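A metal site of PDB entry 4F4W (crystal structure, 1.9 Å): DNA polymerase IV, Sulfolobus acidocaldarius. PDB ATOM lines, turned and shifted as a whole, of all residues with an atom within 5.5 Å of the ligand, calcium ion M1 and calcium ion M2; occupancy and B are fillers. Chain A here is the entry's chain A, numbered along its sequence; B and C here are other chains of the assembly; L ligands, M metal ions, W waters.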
ATOM      1  N   ASP A   7      -3.124  -0.042  20.634  1.00  0.00           N
ATOM      2  CA  ASP A   7      -3.779   0.890  19.735  1.00  0.00           C
ATOM      3  C   ASP A   7      -2.747   1.958  19.376  1.00  0.00           C
ATOM      4  O   ASP A   7      -2.226   2.636  20.269  1.00  0.00           O
ATOM      5  CB  ASP A   7      -4.976   1.498  20.429  1.00  0.00           C
ATOM      6  CG  ASP A   7      -5.872   2.298  19.486  1.00  0.00           C
ATOM      7  OD1 ASP A   7      -7.111   2.230  19.607  1.00  0.00           O
ATOM      8  OD2 ASP A   7      -5.352   3.022  18.669  1.00  0.00           O
ATOM      9  N   PHE A   8      -2.389   2.077  18.091  1.00  0.00           N
ATOM     10  CA  PHE A   8      -1.244   2.914  17.706  1.00  0.00           C
ATOM     11  C   PHE A   8      -1.628   4.404  17.847  1.00  0.00           C
ATOM     12  O   PHE A   8      -2.716   4.788  17.481  1.00  0.00           O
ATOM     13  CB  PHE A   8      -0.781   2.635  16.261  1.00  0.00           C
ATOM     14  CG  PHE A   8      -0.527   1.176  15.954  1.00  0.00           C
ATOM     15  CD1 PHE A   8      -0.614   0.713  14.643  1.00  0.00           C
ATOM     16  CD2 PHE A   8      -0.223   0.275  16.938  1.00  0.00           C
ATOM     17  CE1 PHE A   8      -0.401  -0.626  14.335  1.00  0.00           C
ATOM     18  CE2 PHE A   8       0.003  -1.070  16.634  1.00  0.00           C
ATOM     19  CZ  PHE A   8      -0.092  -1.511  15.329  1.00  0.00           C
ATOM     20  N   ASP A   9      -0.749   5.272  18.353  1.00  0.00           N
ATOM     21  CA  ASP A   9      -1.170   6.672  18.516  1.00  0.00           C
ATOM     22  C   ASP A   9      -1.250   7.433  17.178  1.00  0.00           C
ATOM     23  O   ASP A   9      -0.345   7.339  16.366  1.00  0.00           O
ATOM     24  CB  ASP A   9      -0.212   7.438  19.447  1.00  0.00           C
ATOM     25  CG  ASP A   9      -0.169   6.874  20.853  1.00  0.00           C
ATOM     26  OD1 ASP A   9       0.906   6.989  21.486  1.00  0.00           O
ATOM     27  OD2 ASP A   9      -1.190   6.304  21.304  1.00  0.00           O
ATOM     28  N   TYR A  10      -2.330   8.208  16.994  1.00  0.00           N
ATOM     29  CA  TYR A  10      -2.562   9.093  15.822  1.00  0.00           C
ATOM     30  C   TYR A  10      -1.959   8.514  14.560  1.00  0.00           C
ATOM     31  O   TYR A  10      -1.139   9.154  13.853  1.00  0.00           O
ATOM     32  CB  TYR A  10      -2.134  10.563  16.082  1.00  0.00           C
ATOM     33  CG  TYR A  10      -0.649  10.855  16.328  1.00  0.00           C
ATOM     34  CD1 TYR A  10       0.117  11.500  15.372  1.00  0.00           C
ATOM     35  CD2 TYR A  10      -0.051  10.545  17.547  1.00  0.00           C
ATOM     36  CE1 TYR A  10       1.475  11.801  15.615  1.00  0.00           C
ATOM     37  CE2 TYR A  10       1.303  10.816  17.781  1.00  0.00           C
ATOM     38  CZ  TYR A  10       2.045  11.436  16.816  1.00  0.00           C
ATOM     39  OH  TYR A  10       3.360  11.736  17.058  1.00  0.00           O
ATOM     40  N   PHE A  11      -2.352   7.261  14.293  1.00  0.00           N
ATOM     41  CA  PHE A  11      -1.518   6.367  13.482  1.00  0.00           C
ATOM     42  C   PHE A  11      -1.010   6.921  12.147  1.00  0.00           C
ATOM     43  O   PHE A  11       0.221   7.024  11.938  1.00  0.00           O
ATOM     44  CB  PHE A  11      -2.179   4.997  13.306  1.00  0.00           C
ATOM     45  CG  PHE A  11      -1.301   4.001  12.598  1.00  0.00           C
ATOM     46  CD1 PHE A  11       0.052   3.854  12.950  1.00  0.00           C
ATOM     47  CD2 PHE A  11      -1.827   3.182  11.604  1.00  0.00           C
ATOM     48  CE1 PHE A  11       0.860   2.934  12.281  1.00  0.00           C
ATOM     49  CE2 PHE A  11      -1.014   2.250  10.952  1.00  0.00           C
ATOM     50  CZ  PHE A  11       0.324   2.129  11.288  1.00  0.00           C
ATOM     51  N   PHE A  12      -1.905   7.287  11.232  1.00  0.00           N
ATOM     52  CA  PHE A  12      -1.440   7.676   9.904  1.00  0.00           C
ATOM     53  C   PHE A  12      -0.547   8.919   9.963  1.00  0.00           C
ATOM     54  O   PHE A  12       0.445   9.002   9.241  1.00  0.00           O
ATOM     55  CB  PHE A  12      -2.593   7.970   8.918  1.00  0.00           C
ATOM     56  CG  PHE A  12      -3.454   6.794   8.577  1.00  0.00           C
ATOM     57  CD1 PHE A  12      -3.256   5.524   9.119  1.00  0.00           C
ATOM     58  CD2 PHE A  12      -4.505   6.979   7.682  1.00  0.00           C
ATOM     59  CE1 PHE A  12      -4.084   4.482   8.803  1.00  0.00           C
ATOM     60  CE2 PHE A  12      -5.310   5.948   7.340  1.00  0.00           C
ATOM     61  CZ  PHE A  12      -5.126   4.681   7.902  1.00  0.00           C
ATOM     62  N   ALA A  13      -0.903   9.894  10.807  1.00  0.00           N
ATOM     63  CA  ALA A  13      -0.097  11.108  10.924  1.00  0.00           C
ATOM     64  C   ALA A  13       1.261  10.794  11.548  1.00  0.00           C
ATOM     65  O   ALA A  13       2.277  11.358  11.144  1.00  0.00           O
ATOM     66  CB  ALA A  13      -0.835  12.210  11.754  1.00  0.00           C
ATOM     67  N   VAL A  43     -10.682  14.467   6.308  1.00  0.00           N
ATOM     68  CA  VAL A  43      -9.493  14.221   7.114  1.00  0.00           C
ATOM     69  C   VAL A  43      -9.535  12.779   7.582  1.00  0.00           C
ATOM     70  O   VAL A  43     -10.536  12.351   8.144  1.00  0.00           O
ATOM     71  CB  VAL A  43      -9.505  15.120   8.355  1.00  0.00           C
ATOM     72  CG1 VAL A  43      -8.408  14.708   9.338  1.00  0.00           C
ATOM     73  CG2 VAL A  43      -9.341  16.576   7.934  1.00  0.00           C
ATOM     74  N   ALA A  44      -8.446  12.053   7.351  1.00  0.00           N
ATOM     75  CA  ALA A  44      -8.294  10.688   7.889  1.00  0.00           C
ATOM     76  C   ALA A  44      -7.829  10.758   9.341  1.00  0.00           C
ATOM     77  O   ALA A  44      -8.338  10.038  10.221  1.00  0.00           O
ATOM     78  CB  ALA A  44      -7.275   9.861   7.055  1.00  0.00           C
ATOM     79  N   THR A  45      -6.832  11.596   9.607  1.00  0.00           N
ATOM     80  CA  THR A  45      -6.456  11.828  10.976  1.00  0.00           C
ATOM     81  C   THR A  45      -5.547  13.023  11.084  1.00  0.00           C
ATOM     82  O   THR A  45      -4.993  13.499  10.074  1.00  0.00           O
ATOM     83  CB  THR A  45      -5.849  10.602  11.597  1.00  0.00           C
ATOM     84  OG1 THR A  45      -5.937  10.693  13.038  1.00  0.00           O
ATOM     85  CG2 THR A  45      -4.413  10.444  11.169  1.00  0.00           C
ATOM     86  N   ALA A  46      -5.415  13.508  12.307  1.00  0.00           N
ATOM     87  CA  ALA A  46      -4.551  14.663  12.567  1.00  0.00           C
ATOM     88  C   ALA A  46      -3.706  14.330  13.766  1.00  0.00           C
ATOM     89  O   ALA A  46      -4.150  13.592  14.650  1.00  0.00           O
ATOM     90  CB  ALA A  46      -5.385  15.883  12.861  1.00  0.00           C
ATOM     91  N   TYR A  48      -1.808  15.356  17.378  1.00  0.00           N
ATOM     92  CA  TYR A  48      -2.446  15.987  18.535  1.00  0.00           C
ATOM     93  C   TYR A  48      -2.358  17.518  18.476  1.00  0.00           C
ATOM     94  O   TYR A  48      -3.285  18.197  18.904  1.00  0.00           O
ATOM     95  CB  TYR A  48      -1.859  15.424  19.829  1.00  0.00           C
ATOM     96  CG  TYR A  48      -2.014  13.914  19.938  1.00  0.00           C
ATOM     97  CD1 TYR A  48      -3.174  13.288  19.521  1.00  0.00           C
ATOM     98  CD2 TYR A  48      -0.974  13.123  20.405  1.00  0.00           C
ATOM     99  CE1 TYR A  48      -3.322  11.912  19.611  1.00  0.00           C
ATOM    100  CE2 TYR A  48      -1.111  11.754  20.496  1.00  0.00           C
ATOM    101  CZ  TYR A  48      -2.298  11.165  20.090  1.00  0.00           C
ATOM    102  OH  TYR A  48      -2.437   9.788  20.176  1.00  0.00           O
ATOM    103  N   ARG A  51      -5.196  18.535  16.437  1.00  0.00           N
ATOM    104  CA  ARG A  51      -6.431  18.336  17.167  1.00  0.00           C
ATOM    105  C   ARG A  51      -6.701  19.484  18.161  1.00  0.00           C
ATOM    106  O   ARG A  51      -7.842  19.866  18.414  1.00  0.00           O
ATOM    107  CB  ARG A  51      -6.436  16.983  17.893  1.00  0.00           C
ATOM    108  CG  ARG A  51      -6.542  15.786  16.947  1.00  0.00           C
ATOM    109  CD  ARG A  51      -6.508  14.488  17.688  1.00  0.00           C
ATOM    110  NE  ARG A  51      -6.049  13.411  16.813  1.00  0.00           N
ATOM    111  CZ  ARG A  51      -6.096  12.129  17.131  1.00  0.00           C
ATOM    112  NH1 ARG A  51      -6.570  11.770  18.304  1.00  0.00           N
ATOM    113  NH2 ARG A  51      -5.675  11.208  16.255  1.00  0.00           N
ATOM    114  N   ALA A  57     -10.879  13.763  12.753  1.00  0.00           N
ATOM    115  CA  ALA A  57     -11.041  12.752  11.692  1.00  0.00           C
ATOM    116  C   ALA A  57     -12.454  12.839  11.137  1.00  0.00           C
ATOM    117  O   ALA A  57     -13.397  13.001  11.896  1.00  0.00           O
ATOM    118  CB  ALA A  57     -10.790  11.342  12.243  1.00  0.00           C
ATOM    119  N   GLY A  58     -12.589  12.711   9.818  1.00  0.00           N
ATOM    120  CA  GLY A  58     -13.896  12.694   9.178  1.00  0.00           C
ATOM    121  C   GLY A  58     -14.321  14.069   8.709  1.00  0.00           C
ATOM    122  O   GLY A  58     -15.228  14.223   7.899  1.00  0.00           O
ATOM    123  N   MET A  76      -3.172  11.041   1.961  1.00  0.00           N
ATOM    124  CA  MET A  76      -3.113   9.751   2.624  1.00  0.00           C
ATOM    125  C   MET A  76      -2.251   8.825   1.741  1.00  0.00           C
ATOM    126  O   MET A  76      -2.403   8.806   0.521  1.00  0.00           O
ATOM    127  CB  MET A  76      -4.562   9.241   2.809  1.00  0.00           C
ATOM    128  CG  MET A  76      -4.756   8.213   3.951  1.00  0.00           C
ATOM    129  SD  MET A  76      -6.246   7.244   3.826  1.00  0.00           S
ATOM    130  CE  MET A  76      -6.552   7.199   2.033  1.00  0.00           C
ATOM    131  N   SER A 103      -8.001  -4.095  13.498  1.00  0.00           N
ATOM    132  CA  SER A 103      -8.066  -3.044  12.495  1.00  0.00           C
ATOM    133  C   SER A 103      -6.636  -2.747  12.082  1.00  0.00           C
ATOM    134  O   SER A 103      -5.721  -3.380  12.577  1.00  0.00           O
ATOM    135  CB  SER A 103      -8.746  -1.757  13.019  1.00  0.00           C
ATOM    136  OG  SER A 103      -7.887  -0.916  13.780  1.00  0.00           O
ATOM    137  N   ILE A 104      -6.447  -1.799  11.178  1.00  0.00           N
ATOM    138  CA  ILE A 104      -5.099  -1.452  10.739  1.00  0.00           C
ATOM    139  C   ILE A 104      -4.220  -0.959  11.893  1.00  0.00           C
ATOM    140  O   ILE A 104      -2.984  -0.943  11.798  1.00  0.00           O
ATOM    141  CB  ILE A 104      -5.145  -0.376   9.634  1.00  0.00           C
ATOM    142  CG1 ILE A 104      -3.750  -0.247   9.007  1.00  0.00           C
ATOM    143  CG2 ILE A 104      -5.698   0.953  10.159  1.00  0.00           C
ATOM    144  CD1 ILE A 104      -3.725   0.638   7.814  1.00  0.00           C
ATOM    145  N   ASP A 105      -4.813  -0.497  12.975  1.00  0.00           N
ATOM    146  CA  ASP A 105      -3.934  -0.027  14.035  1.00  0.00           C
ATOM    147  C   ASP A 105      -4.231  -0.513  15.429  1.00  0.00           C
ATOM    148  O   ASP A 105      -3.772   0.097  16.395  1.00  0.00           O
ATOM    149  CB  ASP A 105      -3.804   1.487  14.040  1.00  0.00           C
ATOM    150  CG  ASP A 105      -4.893   2.152  14.830  1.00  0.00           C
ATOM    151  OD1 ASP A 105      -6.005   1.618  14.889  1.00  0.00           O
ATOM    152  OD2 ASP A 105      -4.636   3.231  15.359  1.00  0.00           O
ATOM    153  N   GLU A 106      -4.953  -1.624  15.553  1.00  0.00           N
ATOM    154  CA  GLU A 106      -5.132  -2.165  16.893  1.00  0.00           C
ATOM    155  C   GLU A 106      -5.262  -3.688  16.921  1.00  0.00           C
ATOM    156  O   GLU A 106      -5.755  -4.322  15.949  1.00  0.00           O
ATOM    157  CB  GLU A 106      -6.282  -1.452  17.597  1.00  0.00           C
ATOM    158  CG  GLU A 106      -7.616  -1.765  17.082  1.00  0.00           C
ATOM    159  CD  GLU A 106      -8.708  -0.877  17.665  1.00  0.00           C
ATOM    160  OE1 GLU A 106      -8.622   0.348  17.587  1.00  0.00           O
ATOM    161  OE2 GLU A 106      -9.663  -1.406  18.215  1.00  0.00           O
ATOM    162  N   LYS A 153      -9.487  -2.509  26.156  1.00  0.00           N
ATOM    163  CA  LYS A 153      -9.725  -1.375  25.257  1.00  0.00           C
ATOM    164  C   LYS A 153     -10.115  -0.129  26.016  1.00  0.00           C
ATOM    165  O   LYS A 153      -9.563   0.938  25.800  1.00  0.00           O
ATOM    166  CB  LYS A 153     -10.798  -1.707  24.208  1.00  0.00           C
ATOM    167  CG  LYS A 153     -11.083  -0.573  23.235  1.00  0.00           C
ATOM    168  CD  LYS A 153     -12.070  -1.057  22.200  1.00  0.00           C
ATOM    169  CE  LYS A 153     -12.186  -0.106  21.051  1.00  0.00           C
ATOM    170  NZ  LYS A 153     -11.011  -0.281  20.170  1.00  0.00           N
ATOM    171  N   LYS A 160      -4.645   7.327  26.573  1.00  0.00           N
ATOM    172  CA  LYS A 160      -4.002   7.911  25.383  1.00  0.00           C
ATOM    173  C   LYS A 160      -3.525   9.320  25.698  1.00  0.00           C
ATOM    174  O   LYS A 160      -4.154  10.029  26.473  1.00  0.00           O
ATOM    175  CB  LYS A 160      -4.966   7.976  24.192  1.00  0.00           C
ATOM    176  CG  LYS A 160      -5.392   6.638  23.617  1.00  0.00           C
ATOM    177  CD  LYS A 160      -6.114   6.793  22.234  1.00  0.00           C
ATOM    178  CE  LYS A 160      -6.625   5.452  21.660  1.00  0.00           C
ATOM    179  NZ  LYS A 160      -7.528   5.541  20.428  1.00  0.00           N
ATOM    180  P    DG B   5     -15.578  14.382  -1.050  1.00  0.00           P
ATOM    181  OP1  DG B   5     -15.095  15.083  -2.283  1.00  0.00           O
ATOM    182  OP2  DG B   5     -16.914  13.727  -1.021  1.00  0.00           O
ATOM    183  O5'  DG B   5     -14.382  13.397  -0.700  1.00  0.00           O
ATOM    184  C5'  DG B   5     -14.349  12.749   0.557  1.00  0.00           C
ATOM    185  C4'  DG B   5     -13.222  11.746   0.456  1.00  0.00           C
ATOM    186  O4'  DG B   5     -12.898  11.209   1.752  1.00  0.00           O
ATOM    187  C3'  DG B   5     -13.627  10.522  -0.375  1.00  0.00           C
ATOM    188  O3'  DG B   5     -12.465  10.019  -0.993  1.00  0.00           O
ATOM    189  C2'  DG B   5     -14.245   9.609   0.694  1.00  0.00           C
ATOM    190  C1'  DG B   5     -13.250   9.802   1.833  1.00  0.00           C
ATOM    191  N9   DG B   5     -13.765   9.772   3.209  1.00  0.00           N
ATOM    192  C8   DG B   5     -14.918  10.346   3.696  1.00  0.00           C
ATOM    193  N7   DG B   5     -15.025  10.226   5.002  1.00  0.00           N
ATOM    194  C5   DG B   5     -13.857   9.551   5.372  1.00  0.00           C
ATOM    195  C6   DG B   5     -13.379   9.174   6.645  1.00  0.00           C
ATOM    196  O6   DG B   5     -13.943   9.352   7.740  1.00  0.00           O
ATOM    197  N1   DG B   5     -12.133   8.536   6.593  1.00  0.00           N
ATOM    198  C2   DG B   5     -11.418   8.305   5.448  1.00  0.00           C
ATOM    199  N2   DG B   5     -10.206   7.677   5.543  1.00  0.00           N
ATOM    200  N3   DG B   5     -11.855   8.685   4.266  1.00  0.00           N
ATOM    201  C4   DG B   5     -13.068   9.306   4.295  1.00  0.00           C
ATOM    202  P    DG B   6     -12.551   8.950  -2.198  1.00  0.00           P
ATOM    203  OP1  DG B   6     -11.325   9.098  -3.013  1.00  0.00           O
ATOM    204  OP2  DG B   6     -13.923   9.017  -2.756  1.00  0.00           O
ATOM    205  O5'  DG B   6     -12.422   7.568  -1.421  1.00  0.00           O
ATOM    206  C5'  DG B   6     -11.213   7.310  -0.771  1.00  0.00           C
ATOM    207  C4'  DG B   6     -11.341   6.076   0.082  1.00  0.00           C
ATOM    208  O4'  DG B   6     -11.997   6.429   1.298  1.00  0.00           O
ATOM    209  C3'  DG B   6     -12.180   4.930  -0.537  1.00  0.00           C
ATOM    210  O3'  DG B   6     -11.366   3.787  -0.307  1.00  0.00           O
ATOM    211  C2'  DG B   6     -13.436   4.927   0.367  1.00  0.00           C
ATOM    212  C1'  DG B   6     -12.801   5.371   1.706  1.00  0.00           C
ATOM    213  N9   DG B   6     -13.712   5.823   2.755  1.00  0.00           N
ATOM    214  C8   DG B   6     -14.897   6.487   2.614  1.00  0.00           C
ATOM    215  N7   DG B   6     -15.512   6.718   3.740  1.00  0.00           N
ATOM    216  C5   DG B   6     -14.665   6.189   4.679  1.00  0.00           C
ATOM    217  C6   DG B   6     -14.795   6.154   6.068  1.00  0.00           C
ATOM    218  O6   DG B   6     -15.738   6.593   6.683  1.00  0.00           O
ATOM    219  N1   DG B   6     -13.736   5.501   6.706  1.00  0.00           N
ATOM    220  C2   DG B   6     -12.667   4.976   6.064  1.00  0.00           C
ATOM    221  N2   DG B   6     -11.736   4.374   6.821  1.00  0.00           N
ATOM    222  N3   DG B   6     -12.543   5.023   4.751  1.00  0.00           N
ATOM    223  C4   DG B   6     -13.571   5.620   4.112  1.00  0.00           C
ATOM    224  P    DC C  13     -13.930   2.721  17.050  1.00  0.00           P
ATOM    225  OP1  DC C  13     -13.459   1.611  17.916  1.00  0.00           O
ATOM    226  OP2  DC C  13     -14.159   4.124  17.526  1.00  0.00           O
ATOM    227  O5'  DC C  13     -12.844   2.769  15.861  1.00  0.00           O
ATOM    228  C5'  DC C  13     -12.289   1.548  15.337  1.00  0.00           C
ATOM    229  C4'  DC C  13     -11.580   1.952  14.044  1.00  0.00           C
ATOM    230  O4'  DC C  13     -12.536   2.605  13.180  1.00  0.00           O
ATOM    231  C3'  DC C  13     -10.566   3.019  14.345  1.00  0.00           C
ATOM    232  O3'  DC C  13      -9.282   2.407  14.556  1.00  0.00           O
ATOM    233  C2'  DC C  13     -10.689   4.029  13.202  1.00  0.00           C
ATOM    234  C1'  DC C  13     -11.777   3.437  12.313  1.00  0.00           C
ATOM    235  N1   DC C  13     -12.742   4.353  11.593  1.00  0.00           N
ATOM    236  C2   DC C  13     -12.762   4.439  10.163  1.00  0.00           C
ATOM    237  O2   DC C  13     -11.942   3.788   9.509  1.00  0.00           O
ATOM    238  N3   DC C  13     -13.644   5.265   9.568  1.00  0.00           N
ATOM    239  C4   DC C  13     -14.513   5.969  10.289  1.00  0.00           C
ATOM    240  N4   DC C  13     -15.398   6.764   9.686  1.00  0.00           N
ATOM    241  C5   DC C  13     -14.512   5.897  11.723  1.00  0.00           C
ATOM    242  C6   DC C  13     -13.626   5.083  12.300  1.00  0.00           C
HETATM  243  N1  LIG L   1      -9.094   6.596  10.210  1.00  0.00           N
HETATM  244  C1  LIG L   1      -9.686   7.027   9.064  1.00  0.00           C
HETATM  245  N2  LIG L   1     -10.849   7.686   9.053  1.00  0.00           N
HETATM  246  C2  LIG L   1     -11.433   7.957  10.236  1.00  0.00           C
HETATM  247  C3  LIG L   1     -10.863   7.556  11.437  1.00  0.00           C
HETATM  248  C4  LIG L   1      -9.648   6.866  11.421  1.00  0.00           C
HETATM  249  O1  LIG L   1      -9.087   6.794   7.891  1.00  0.00           O
HETATM  250  N3  LIG L   1     -12.675   8.675  10.295  1.00  0.00           N
HETATM  251  C5  LIG L   1      -7.802   5.917  10.203  1.00  0.00           C
HETATM  252  C6  LIG L   1      -6.733   6.912  10.483  1.00  0.00           C
HETATM  253  C7  LIG L   1      -6.361   6.635  11.904  1.00  0.00           C
HETATM  254  C8  LIG L   1      -6.581   5.222  12.002  1.00  0.00           C
HETATM  255  O2  LIG L   1      -7.776   4.965  11.239  1.00  0.00           O
HETATM  256  O3  LIG L   1      -5.031   7.025  12.245  1.00  0.00           O
HETATM  257  C9  LIG L   1      -6.812   4.818  13.396  1.00  0.00           C
HETATM  258  O4  LIG L   1      -7.961   5.404  13.955  1.00  0.00           O
HETATM  259  P1  LIG L   1      -8.038   5.810  15.471  1.00  0.00           P
HETATM  260  O5  LIG L   1      -9.480   5.938  15.852  1.00  0.00           O
HETATM  261  O6  LIG L   1      -7.428   4.773  16.306  1.00  0.00           O
HETATM  262  O7  LIG L   1      -7.331   7.198  15.657  1.00  0.00           O
HETATM  263  P2  LIG L   1      -5.821   7.616  15.628  1.00  0.00           P
HETATM  264  O8  LIG L   1      -4.860   6.506  15.604  1.00  0.00           O
HETATM  265  O9  LIG L   1      -5.581   8.461  14.414  1.00  0.00           O
HETATM  266  O10 LIG L   1      -5.634   8.562  16.890  1.00  0.00           O
HETATM  267  P3  LIG L   1      -5.647   8.037  18.406  1.00  0.00           P
HETATM  268  O11 LIG L   1      -4.311   8.418  18.983  1.00  0.00           O
HETATM  269  O12 LIG L   1      -6.683   8.852  19.096  1.00  0.00           O
HETATM  270  O13 LIG L   1      -5.915   6.525  18.524  1.00  0.00           O
HETATM  271 CA    CA M   1      -7.796   2.513  16.895  1.00  0.00          CA
HETATM  272 CA    CA M   2      -5.094   4.709  17.207  1.00  0.00          CA
HETATM  273  O   HOH W   1      -8.204   9.587  13.155  1.00  0.00           O
HETATM  274  O   HOH W   2      -3.931   5.310  20.271  1.00  0.00           O
HETATM  275  O   HOH W   3      -6.708  10.148  21.543  1.00  0.00           O
HETATM  276  O   HOH W   4      -8.453   4.734   6.290  1.00  0.00           O
HETATM  277  O   HOH W   5     -10.430   8.520  14.632  1.00  0.00           O
HETATM  278  O   HOH W   6      -9.411   3.367  17.930  1.00  0.00           O
HETATM  279  O   HOH W   7      -9.484   9.283  18.629  1.00  0.00           O
HETATM  280  O   HOH W   8     -14.070   9.320  12.797  1.00  0.00           O
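An oxygen (O3) of the ligand is in hydrogen-bond range of the backbone NH of Phe 11, 3.4 Å away. The backbone NH (N) of Phe 12 lies within hydrogen-bond range of an oxygen (O3) of the ligand (3.3 Å). The guanidinium group (NH1) of Arg 51 lies within salt-bridge range of an oxygen (O12) of the ligand. O9 of the ligand sits at hydrogen-bond distance from OG1 of Thr 45, 2.6 Å away. N4 of DC 13 of chain C lies close to a nitrogen (N3) of the ligand. The side-chain amino group of Lys 160 is in salt-bridge range of an oxygen (O12) of the ligand (3.7 Å). A nitrogen (N3) of the ligand lies within hydrogen-bond range of O6 of DG 5 of chain B, at 2.9 Å. N of Tyr 10 is in hydrogen-bond range of O11 of the ligand (2.8 Å). O11 of the ligand sits at hydrogen-bond distance from OH of Tyr 48, 2.6 Å away.
Three residues have an atom within 4 Å of calcium ion M2: Asp 7, Phe 8 and Asp 105.
The backbone NH of Asp 105 sits close to the side-chain hydroxyl of Ser 103, 3.2 Å away. The side-chain hydroxyl (OG1) of Thr 45 sits at hydrogen-bond distance from the guanidinium group (NH2) of Arg 51, 3.3 Å away. The guanidinium group of Arg 51 lies within hydrogen-bond range of the backbone carbonyl oxygen of Ala 46 (2.9 Å). OP1 of DC 13 of chain C is in salt-bridge range of NZ of Lys 153 (3.8 Å). The side-chain carboxylate (OD1) of Asp 7 lies close to the side-chain amino group (NZ) of Lys 160, at 3.4 Å. OE2 of Glu 106 lies within salt-bridge range of NZ of Lys 153, at 2.6 Å.
Of the 25 residues printed, 4 come within 4 Å of calcium ion M1.
Calcium ion M1 is bound by water W6 (2.1 Å), O6 of the ligand (2.4 Å), OE1 of Glu 106 (2.4 Å), O3' of DC 13 of chain C (2.8 Å), OD1 of Asp 7 (2.8 Å) and OD1 of Asp 105 (2.8 Å). Slightly farther from calcium ion M1 lies the side-chain carboxylate (OD2) of Asp 7 (3.1 Å).
Residues that only touch the ligand: Ala 44, Asp 9, DG 6 of chain B and Ala 57. Hydrophobic or aromatic side chains within 4 Å of the ligand: Phe 11, Phe 12, Ala 44, Tyr 48 and Ala 57. 16 residues have an atom within 4 Å of the ligand: Asp 7, Phe 8, Asp 9, Tyr 10, Phe 11, Phe 12, Ala 44, Thr 45, Tyr 48, Arg 51, Ala 57, Asp 105, Lys 160, DG 5 of chain B, DG 6 of chain B and DC 13 of chain C.
Calcium ion M2 is bound by the side-chain carboxylate (OD2) of Asp 7 (2.2 Å), an oxygen (O13) of the ligand (2.4 Å), the backbone carbonyl oxygen (O) of Phe 8 (2.4 Å), the side-chain carboxylate (OD2) of Asp 105 (2.4 Å), an oxygen (O8) of the ligand (2.4 Å) and an oxygen (O6) of the ligand (2.5 Å).
Water W4 bridges an oxygen (O1) of the ligand (2.7 Å) and N2 of DG 6 of chain B (3.3 Å). Water W2 lies within hydrogen-bond range of OD2 of Asp 9, O of Asp 7 and O11 of the ligand. Water W1 lies within hydrogen-bond range of OG1 of Thr 45 (2.5 Å), O of Ala 44 (3.0 Å) and O9 of the ligand (3.1 Å).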
